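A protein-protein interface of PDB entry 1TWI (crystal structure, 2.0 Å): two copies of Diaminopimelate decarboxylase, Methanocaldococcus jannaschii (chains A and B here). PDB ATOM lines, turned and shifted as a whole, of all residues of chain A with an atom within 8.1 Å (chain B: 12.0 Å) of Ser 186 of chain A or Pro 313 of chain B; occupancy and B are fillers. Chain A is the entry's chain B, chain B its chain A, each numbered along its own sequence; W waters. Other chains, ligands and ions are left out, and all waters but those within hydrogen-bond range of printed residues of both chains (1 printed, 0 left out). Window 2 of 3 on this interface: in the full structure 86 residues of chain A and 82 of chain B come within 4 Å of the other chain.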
ATOM      1  N   ASN A 160      13.865  -3.884  -8.037  1.00  0.00           N
ATOM      2  CA  ASN A 160      12.952  -4.380  -7.002  1.00  0.00           C
ATOM      3  C   ASN A 160      11.713  -3.505  -7.165  1.00  0.00           C
ATOM      4  O   ASN A 160      11.628  -2.409  -6.594  1.00  0.00           O
ATOM      5  CB  ASN A 160      13.553  -4.172  -5.630  1.00  0.00           C
ATOM      6  CG  ASN A 160      14.817  -4.973  -5.468  1.00  0.00           C
ATOM      7  OD1 ASN A 160      14.974  -5.966  -6.159  1.00  0.00           O
ATOM      8  ND2 ASN A 160      15.725  -4.557  -4.568  1.00  0.00           N
ATOM      9  N   ASN A 162       7.807  -2.045  -7.096  1.00  0.00           N
ATOM     10  CA  ASN A 162       6.872  -1.723  -6.010  1.00  0.00           C
ATOM     11  C   ASN A 162       5.760  -2.786  -5.850  1.00  0.00           C
ATOM     12  O   ASN A 162       4.569  -2.491  -6.034  1.00  0.00           O
ATOM     13  CB  ASN A 162       6.260  -0.331  -6.281  1.00  0.00           C
ATOM     14  CG  ASN A 162       5.410  -0.300  -7.559  1.00  0.00           C
ATOM     15  OD1 ASN A 162       5.612  -1.118  -8.488  1.00  0.00           O
ATOM     16  ND2 ASN A 162       4.454   0.654  -7.620  1.00  0.00           N
ATOM     17  N   LEU A 175      12.095  -8.735  -1.664  1.00  0.00           N
ATOM     18  CA  LEU A 175      12.564  -7.653  -2.474  1.00  0.00           C
ATOM     19  C   LEU A 175      13.158  -6.515  -1.653  1.00  0.00           C
ATOM     20  O   LEU A 175      14.107  -5.866  -2.114  1.00  0.00           O
ATOM     21  CB  LEU A 175      11.430  -7.123  -3.327  1.00  0.00           C
ATOM     22  CG  LEU A 175      11.162  -7.967  -4.557  1.00  0.00           C
ATOM     23  CD1 LEU A 175       9.777  -7.609  -5.136  1.00  0.00           C
ATOM     24  CD2 LEU A 175      12.294  -7.672  -5.582  1.00  0.00           C
ATOM     25  N   LYS A 176      12.617  -6.250  -0.459  1.00  0.00           N
ATOM     26  CA  LYS A 176      13.161  -5.128   0.298  1.00  0.00           C
ATOM     27  C   LYS A 176      14.349  -5.438   1.199  1.00  0.00           C
ATOM     28  O   LYS A 176      15.335  -4.707   1.203  1.00  0.00           O
ATOM     29  CB  LYS A 176      12.061  -4.464   1.133  1.00  0.00           C
ATOM     30  CG  LYS A 176      10.950  -3.823   0.284  1.00  0.00           C
ATOM     31  CD  LYS A 176      10.078  -2.919   1.131  1.00  0.00           C
ATOM     32  CE  LYS A 176       8.903  -2.331   0.292  1.00  0.00           C
ATOM     33  NZ  LYS A 176       7.900  -1.547   1.144  1.00  0.00           N
ATOM     34  N   LYS A 177      14.266  -6.540   1.928  1.00  0.00           N
ATOM     35  CA  LYS A 177      15.315  -6.896   2.868  1.00  0.00           C
ATOM     36  C   LYS A 177      16.475  -7.749   2.309  1.00  0.00           C
ATOM     37  O   LYS A 177      17.526  -7.899   2.964  1.00  0.00           O
ATOM     38  CB  LYS A 177      14.684  -7.634   4.060  1.00  0.00           C
ATOM     39  CG  LYS A 177      14.233  -9.066   3.768  1.00  0.00           C
ATOM     40  CD  LYS A 177      13.714  -9.774   5.067  1.00  0.00           C
ATOM     41  CE  LYS A 177      13.568 -11.315   4.902  1.00  0.00           C
ATOM     42  NZ  LYS A 177      12.642 -11.966   5.920  1.00  0.00           N
ATOM     43  N   GLY A 181      19.216  -6.348  -6.191  1.00  0.00           N
ATOM     44  CA  GLY A 181      18.445  -5.338  -6.896  1.00  0.00           C
ATOM     45  C   GLY A 181      18.534  -3.893  -6.485  1.00  0.00           C
ATOM     46  O   GLY A 181      19.101  -3.563  -5.441  1.00  0.00           O
ATOM     47  N   LEU A 182      17.960  -3.050  -7.344  1.00  0.00           N
ATOM     48  CA  LEU A 182      17.912  -1.601  -7.149  1.00  0.00           C
ATOM     49  C   LEU A 182      16.443  -1.273  -6.819  1.00  0.00           C
ATOM     50  O   LEU A 182      15.520  -1.528  -7.627  1.00  0.00           O
ATOM     51  CB  LEU A 182      18.339  -0.896  -8.440  1.00  0.00           C
ATOM     52  CG  LEU A 182      19.808  -1.143  -8.834  1.00  0.00           C
ATOM     53  CD1 LEU A 182      19.890  -1.244 -10.369  1.00  0.00           C
ATOM     54  CD2 LEU A 182      20.763  -0.007  -8.342  1.00  0.00           C
ATOM     55  N   ASP A 183      16.234  -0.708  -5.636  1.00  0.00           N
ATOM     56  CA  ASP A 183      14.897  -0.361  -5.168  1.00  0.00           C
ATOM     57  C   ASP A 183      14.236   0.687  -6.079  1.00  0.00           C
ATOM     58  O   ASP A 183      14.843   1.702  -6.422  1.00  0.00           O
ATOM     59  CB  ASP A 183      15.003   0.171  -3.727  1.00  0.00           C
ATOM     60  CG  ASP A 183      13.646   0.391  -3.084  1.00  0.00           C
ATOM     61  OD1 ASP A 183      13.289   1.569  -2.914  1.00  0.00           O
ATOM     62  OD2 ASP A 183      12.958  -0.623  -2.771  1.00  0.00           O
ATOM     63  N   VAL A 184      13.012   0.413  -6.504  1.00  0.00           N
ATOM     64  CA  VAL A 184      12.317   1.356  -7.360  1.00  0.00           C
ATOM     65  C   VAL A 184      11.644   2.447  -6.513  1.00  0.00           C
ATOM     66  O   VAL A 184      11.854   3.644  -6.730  1.00  0.00           O
ATOM     67  CB  VAL A 184      11.216   0.691  -8.187  1.00  0.00           C
ATOM     68  CG1 VAL A 184      10.416   1.772  -8.885  1.00  0.00           C
ATOM     69  CG2 VAL A 184      11.826  -0.244  -9.269  1.00  0.00           C
ATOM     70  N   GLU A 185      10.844   2.016  -5.545  1.00  0.00           N
ATOM     71  CA  GLU A 185      10.129   2.949  -4.663  1.00  0.00           C
ATOM     72  C   GLU A 185      10.948   4.172  -4.226  1.00  0.00           C
ATOM     73  O   GLU A 185      10.505   5.297  -4.375  1.00  0.00           O
ATOM     74  CB  GLU A 185       9.633   2.209  -3.408  1.00  0.00           C
ATOM     75  CG  GLU A 185       8.978   3.132  -2.396  1.00  0.00           C
ATOM     76  CD  GLU A 185       8.366   2.375  -1.230  1.00  0.00           C
ATOM     77  OE1 GLU A 185       7.556   2.993  -0.473  1.00  0.00           O
ATOM     78  OE2 GLU A 185       8.693   1.162  -1.062  1.00  0.00           O
ATOM     79  N   SER A 186      12.137   3.941  -3.694  1.00  0.00           N
ATOM     80  CA  SER A 186      13.033   4.981  -3.178  1.00  0.00           C
ATOM     81  C   SER A 186      13.736   5.847  -4.218  1.00  0.00           C
ATOM     82  O   SER A 186      14.484   6.785  -3.859  1.00  0.00           O
ATOM     83  CB  SER A 186      14.129   4.312  -2.337  1.00  0.00           C
ATOM     84  OG  SER A 186      15.033   3.640  -3.223  1.00  0.00           O
ATOM     85  N   GLY A 187      13.540   5.542  -5.498  1.00  0.00           N
ATOM     86  CA  GLY A 187      14.218   6.317  -6.528  1.00  0.00           C
ATOM     87  C   GLY A 187      15.609   5.792  -6.898  1.00  0.00           C
ATOM     88  O   GLY A 187      16.276   6.321  -7.787  1.00  0.00           O
ATOM     89  N   ILE A 188      16.070   4.725  -6.263  1.00  0.00           N
ATOM     90  CA  ILE A 188      17.426   4.227  -6.593  1.00  0.00           C
ATOM     91  C   ILE A 188      17.572   3.652  -8.023  1.00  0.00           C
ATOM     92  O   ILE A 188      18.562   3.891  -8.666  1.00  0.00           O
ATOM     93  CB  ILE A 188      17.892   3.191  -5.514  1.00  0.00           C
ATOM     94  CG1 ILE A 188      18.075   3.940  -4.183  1.00  0.00           C
ATOM     95  CG2 ILE A 188      19.225   2.501  -5.931  1.00  0.00           C
ATOM     96  CD1 ILE A 188      18.246   3.059  -2.911  1.00  0.00           C
ATOM     97  N   ALA A 189      16.592   2.903  -8.508  1.00  0.00           N
ATOM     98  CA  ALA A 189      16.657   2.327  -9.859  1.00  0.00           C
ATOM     99  C   ALA A 189      16.684   3.404 -10.944  1.00  0.00           C
ATOM    100  O   ALA A 189      17.470   3.333 -11.881  1.00  0.00           O
ATOM    101  CB  ALA A 189      15.482   1.413 -10.077  1.00  0.00           C
ATOM    102  N   MET A 190      15.835   4.417 -10.813  1.00  0.00           N
ATOM    103  CA  MET A 190      15.819   5.516 -11.800  1.00  0.00           C
ATOM    104  C   MET A 190      17.166   6.242 -11.742  1.00  0.00           C
ATOM    105  O   MET A 190      17.752   6.558 -12.784  1.00  0.00           O
ATOM    106  CB  MET A 190      14.662   6.505 -11.498  1.00  0.00           C
ATOM    107  CG  MET A 190      14.511   7.702 -12.512  1.00  0.00           C
ATOM    108  SD  MET A 190      14.061   7.120 -14.124  1.00  0.00           S
ATOM    109  CE  MET A 190      12.403   6.606 -13.833  1.00  0.00           C
ATOM    110  N   LYS A 191      17.679   6.508 -10.545  1.00  0.00           N
ATOM    111  CA  LYS A 191      18.964   7.211 -10.464  1.00  0.00           C
ATOM    112  C   LYS A 191      20.105   6.404 -11.134  1.00  0.00           C
ATOM    113  O   LYS A 191      21.012   6.945 -11.790  1.00  0.00           O
ATOM    114  CB  LYS A 191      19.309   7.443  -9.009  1.00  0.00           C
ATOM    115  CG  LYS A 191      20.725   7.875  -8.712  1.00  0.00           C
ATOM    116  CD  LYS A 191      20.788   8.092  -7.184  1.00  0.00           C
ATOM    117  CE  LYS A 191      22.229   8.111  -6.623  1.00  0.00           C
ATOM    118  NZ  LYS A 191      22.892   9.427  -6.878  1.00  0.00           N
ATOM    119  N   ILE B 309      30.074  -1.733  -2.005  1.00  0.00           N
ATOM    120  CA  ILE B 309      29.285  -1.281  -0.860  1.00  0.00           C
ATOM    121  C   ILE B 309      27.964  -0.827  -1.484  1.00  0.00           C
ATOM    122  O   ILE B 309      27.941  -0.161  -2.533  1.00  0.00           O
ATOM    123  CB  ILE B 309      29.950  -0.113  -0.108  1.00  0.00           C
ATOM    124  CG1 ILE B 309      31.286  -0.598   0.509  1.00  0.00           C
ATOM    125  CG2 ILE B 309      28.959   0.417   0.963  1.00  0.00           C
ATOM    126  CD1 ILE B 309      32.160   0.479   1.083  1.00  0.00           C
ATOM    127  N   LYS B 310      26.855  -1.168  -0.856  1.00  0.00           N
ATOM    128  CA  LYS B 310      25.545  -0.837  -1.415  1.00  0.00           C
ATOM    129  C   LYS B 310      24.519  -0.339  -0.393  1.00  0.00           C
ATOM    130  O   LYS B 310      24.022  -1.114   0.408  1.00  0.00           O
ATOM    131  CB  LYS B 310      24.988  -2.098  -2.089  1.00  0.00           C
ATOM    132  CG  LYS B 310      23.562  -2.060  -2.561  1.00  0.00           C
ATOM    133  CD  LYS B 310      23.248  -3.403  -3.315  1.00  0.00           C
ATOM    134  CE  LYS B 310      21.871  -3.450  -3.952  1.00  0.00           C
ATOM    135  NZ  LYS B 310      21.437  -4.859  -4.363  1.00  0.00           N
ATOM    136  N   GLU B 311      24.175   0.935  -0.436  1.00  0.00           N
ATOM    137  CA  GLU B 311      23.176   1.443   0.505  1.00  0.00           C
ATOM    138  C   GLU B 311      21.780   1.185  -0.013  1.00  0.00           C
ATOM    139  O   GLU B 311      21.511   1.426  -1.204  1.00  0.00           O
ATOM    140  CB  GLU B 311      23.361   2.935   0.700  1.00  0.00           C
ATOM    141  CG  GLU B 311      24.740   3.226   1.222  1.00  0.00           C
ATOM    142  CD  GLU B 311      24.978   4.685   1.404  1.00  0.00           C
ATOM    143  OE1 GLU B 311      26.057   5.039   1.945  1.00  0.00           O
ATOM    144  OE2 GLU B 311      24.091   5.478   1.006  1.00  0.00           O
ATOM    145  N   THR B 312      20.896   0.652   0.835  1.00  0.00           N
ATOM    146  CA  THR B 312      19.516   0.448   0.405  1.00  0.00           C
ATOM    147  C   THR B 312      18.648   1.140   1.456  1.00  0.00           C
ATOM    148  O   THR B 312      19.130   1.592   2.497  1.00  0.00           O
ATOM    149  CB  THR B 312      19.059  -1.058   0.318  1.00  0.00           C
ATOM    150  OG1 THR B 312      18.865  -1.572   1.645  1.00  0.00           O
ATOM    151  CG2 THR B 312      20.084  -1.938  -0.484  1.00  0.00           C
ATOM    152  N   PRO B 313      17.352   1.231   1.198  1.00  0.00           N
ATOM    153  CA  PRO B 313      16.485   1.887   2.175  1.00  0.00           C
ATOM    154  C   PRO B 313      16.552   1.229   3.550  1.00  0.00           C
ATOM    155  O   PRO B 313      16.528   1.935   4.546  1.00  0.00           O
ATOM    156  CB  PRO B 313      15.100   1.770   1.540  1.00  0.00           C
ATOM    157  CG  PRO B 313      15.405   1.835   0.068  1.00  0.00           C
ATOM    158  CD  PRO B 313      16.617   0.907  -0.036  1.00  0.00           C
ATOM    159  N   VAL B 314      16.668  -0.103   3.604  1.00  0.00           N
ATOM    160  CA  VAL B 314      16.694  -0.809   4.887  1.00  0.00           C
ATOM    161  C   VAL B 314      18.076  -1.222   5.430  1.00  0.00           C
ATOM    162  O   VAL B 314      18.231  -1.430   6.637  1.00  0.00           O
ATOM    163  CB  VAL B 314      15.848  -2.094   4.829  1.00  0.00           C
ATOM    164  CG1 VAL B 314      16.394  -3.013   3.758  1.00  0.00           C
ATOM    165  CG2 VAL B 314      15.909  -2.824   6.170  1.00  0.00           C
ATOM    166  N   THR B 315      19.070  -1.409   4.569  1.00  0.00           N
ATOM    167  CA  THR B 315      20.357  -1.798   5.098  1.00  0.00           C
ATOM    168  C   THR B 315      21.528  -1.462   4.219  1.00  0.00           C
ATOM    169  O   THR B 315      21.393  -1.270   3.003  1.00  0.00           O
ATOM    170  CB  THR B 315      20.398  -3.337   5.513  1.00  0.00           C
ATOM    171  OG1 THR B 315      21.345  -4.057   4.722  1.00  0.00           O
ATOM    172  CG2 THR B 315      19.050  -3.979   5.374  1.00  0.00           C
ATOM    173  N   LYS B 316      22.674  -1.278   4.860  1.00  0.00           N
ATOM    174  CA  LYS B 316      23.870  -1.001   4.084  1.00  0.00           C
ATOM    175  C   LYS B 316      24.587  -2.353   3.957  1.00  0.00           C
ATOM    176  O   LYS B 316      24.977  -2.987   4.945  1.00  0.00           O
ATOM    177  CB  LYS B 316      24.769   0.034   4.762  1.00  0.00           C
ATOM    178  CG  LYS B 316      25.971   0.416   3.910  1.00  0.00           C
ATOM    179  CD  LYS B 316      26.613   1.687   4.501  1.00  0.00           C
ATOM    180  CE  LYS B 316      27.981   1.927   3.889  1.00  0.00           C
ATOM    181  NZ  LYS B 316      28.541   3.300   4.115  1.00  0.00           N
ATOM    182  N   TRP B 317      24.682  -2.806   2.714  1.00  0.00           N
ATOM    183  CA  TRP B 317      25.302  -4.089   2.409  1.00  0.00           C
ATOM    184  C   TRP B 317      26.737  -3.906   1.979  1.00  0.00           C
ATOM    185  O   TRP B 317      27.061  -2.979   1.239  1.00  0.00           O
ATOM    186  CB  TRP B 317      24.586  -4.774   1.263  1.00  0.00           C
ATOM    187  CG  TRP B 317      23.227  -5.269   1.562  1.00  0.00           C
ATOM    188  CD1 TRP B 317      22.016  -4.640   1.309  1.00  0.00           C
ATOM    189  CD2 TRP B 317      22.911  -6.507   2.187  1.00  0.00           C
ATOM    190  NE1 TRP B 317      20.985  -5.438   1.770  1.00  0.00           N
ATOM    191  CE2 TRP B 317      21.520  -6.579   2.309  1.00  0.00           C
ATOM    192  CE3 TRP B 317      23.683  -7.569   2.657  1.00  0.00           C
ATOM    193  CZ2 TRP B 317      20.889  -7.677   2.889  1.00  0.00           C
ATOM    194  CZ3 TRP B 317      23.063  -8.643   3.223  1.00  0.00           C
ATOM    195  CH2 TRP B 317      21.690  -8.695   3.336  1.00  0.00           C
ATOM    196  N   VAL B 318      27.568  -4.828   2.429  1.00  0.00           N
ATOM    197  CA  VAL B 318      28.989  -4.876   2.120  1.00  0.00           C
ATOM    198  C   VAL B 318      29.130  -6.240   1.393  1.00  0.00           C
ATOM    199  O   VAL B 318      28.768  -7.277   1.954  1.00  0.00           O
ATOM    200  CB  VAL B 318      29.772  -4.812   3.481  1.00  0.00           C
ATOM    201  CG1 VAL B 318      31.182  -5.278   3.306  1.00  0.00           C
ATOM    202  CG2 VAL B 318      29.757  -3.343   3.987  1.00  0.00           C
ATOM    203  N   MET B 319      29.601  -6.233   0.136  1.00  0.00           N
ATOM    204  CA  MET B 319      29.700  -7.473  -0.637  1.00  0.00           C
ATOM    205  C   MET B 319      31.138  -7.939  -0.711  1.00  0.00           C
ATOM    206  O   MET B 319      31.999  -7.207  -1.181  1.00  0.00           O
ATOM    207  CB  MET B 319      29.198  -7.262  -2.077  1.00  0.00           C
ATOM    208  CG  MET B 319      27.892  -6.418  -2.211  1.00  0.00           C
ATOM    209  SD  MET B 319      26.520  -7.186  -1.351  1.00  0.00           S
ATOM    210  CE  MET B 319      25.071  -6.322  -2.179  1.00  0.00           C
ATOM    211  N   VAL B 350      27.091   0.205  11.087  1.00  0.00           N
ATOM    212  CA  VAL B 350      26.384  -1.069  11.137  1.00  0.00           C
ATOM    213  C   VAL B 350      26.077  -1.467   9.709  1.00  0.00           C
ATOM    214  O   VAL B 350      25.516  -0.668   8.956  1.00  0.00           O
ATOM    215  CB  VAL B 350      25.047  -0.941  11.927  1.00  0.00           C
ATOM    216  CG1 VAL B 350      24.256  -2.228  11.845  1.00  0.00           C
ATOM    217  CG2 VAL B 350      25.356  -0.596  13.390  1.00  0.00           C
ATOM    218  N   VAL B 351      26.463  -2.688   9.336  1.00  0.00           N
ATOM    219  CA  VAL B 351      26.247  -3.190   7.979  1.00  0.00           C
ATOM    220  C   VAL B 351      25.920  -4.685   7.995  1.00  0.00           C
ATOM    221  O   VAL B 351      26.121  -5.350   9.008  1.00  0.00           O
ATOM    222  CB  VAL B 351      27.527  -3.046   7.070  1.00  0.00           C
ATOM    223  CG1 VAL B 351      27.948  -1.593   6.898  1.00  0.00           C
ATOM    224  CG2 VAL B 351      28.683  -3.858   7.672  1.00  0.00           C
ATOM    225  N   SER B 352      25.423  -5.197   6.866  1.00  0.00           N
ATOM    226  CA  SER B 352      25.148  -6.629   6.703  1.00  0.00           C
ATOM    227  C   SER B 352      26.194  -7.083   5.657  1.00  0.00           C
ATOM    228  O   SER B 352      26.546  -6.337   4.750  1.00  0.00           O
ATOM    229  CB  SER B 352      23.718  -6.847   6.222  1.00  0.00           C
ATOM    230  OG  SER B 352      22.792  -6.515   7.265  1.00  0.00           O
ATOM    231  N   ASP B 367      23.374  -6.651  10.393  1.00  0.00           N
ATOM    232  CA  ASP B 367      23.429  -5.630  11.414  1.00  0.00           C
ATOM    233  C   ASP B 367      24.652  -5.751  12.292  1.00  0.00           C
ATOM    234  O   ASP B 367      24.544  -5.758  13.505  1.00  0.00           O
ATOM    235  CB  ASP B 367      22.159  -5.720  12.250  1.00  0.00           C
ATOM    236  CG  ASP B 367      20.906  -5.589  11.385  1.00  0.00           C
ATOM    237  OD1 ASP B 367      19.908  -6.256  11.676  1.00  0.00           O
ATOM    238  OD2 ASP B 367      20.921  -4.826  10.385  1.00  0.00           O
HETATM  239  O   HOH W   1      18.228  -4.319   1.697  1.00  0.00           O
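The side-chain amino group (NZ) of Lys 310 of chain B sits at hydrogen-bond distance from the backbone carbonyl oxygen (O) of Gly 181 of chain A (2.9 Å).
The backbone NH of Lys 310 of chain B sits at hydrogen-bond distance from the backbone carbonyl oxygen of Trp 317 of chain B. O of Asp 183 of chain A lies within hydrogen-bond range of N of Ala 189 of chain A. The backbone NH (N) of Ile 188 of chain A lies close to the side-chain hydroxyl (OG) of Ser 186 of chain A. The side-chain hydroxyl of Thr 312 of chain B sits close to the backbone NH of Val 314 of chain B, at 3.3 Å. The side-chain carboxylate of Glu 185 of chain A is in salt-bridge range of the side-chain amino group of Lys 176 of chain A. The side-chain carboxylate (OD1) of Asp 183 of chain A is in hydrogen-bond range of the side-chain hydroxyl (OG) of Ser 186 of chain A, at 2.7 Å.
Among the printed residues, merely in contact across the chains: Lys 176 of chain A with Val 314 of chain B, Lys 177 of chain A with Trp 317 of chain B, Asp 183 of chain A with Pro 313 of chain B, Ser 186 of chain A with Pro 313 of chain B and Ile 188 of chain A with Pro 313 of chain B.
Printed residues of chain B within 4 Å of Lys 177 of chain A: Trp 317 (3.4 Å). Of the printed residues of chain B, Asp 183 of chain A touches Pro 313. No residue of chain B comes within 4 Å of Val 184 of chain A. No residue of chain B comes within 4 Å of Glu 185 of chain A. Printed residues of chain B within 4 Å of Ser 186 of chain A: Pro 313 (3.7 Å). Ile 188 of chain A touches just one residue of chain B: Pro 313. Of the printed residues of chain A, Lys 310 of chain B touches Gly 181 (2.9 Å). Of the printed residues of chain A, Pro 313 of chain B touches Asp 183 (3.7 Å), Ser 186 (3.7 Å) and Ile 188 (3.9 Å). Printed residues of chain A within 4 Å of Trp 317 of chain B: Lys 177 (3.4 Å). The nearest residue of chain A that does not touch Pro 313 of chain B is Lys 176 of chain A (5.9 Å).
Of the 16 printed residues of chain A, 6 touch a printed residue of chain B. Printed residues of chain A that touch a printed residue of chain B: Lys 176, Lys 177, Gly 181, Asp 183, Ser 186 and Ile 188. Hydrophobic or aromatic side chains of chain A that line the printed part of chain B: Ile 188.
No position is printed for both chains. Of the 6 pairs that touch across the chains among the printed residues, none has its exchanged pair printed and touching as well.
Water W1 lies within hydrogen-bond range of the side-chain hydroxyl of Thr 312 of chain B (2.8 Å), the backbone carbonyl oxygen of Lys 176 of chain A (3.0 Å) and the indole nitrogen of Trp 317 of chain B (3.0 Å).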
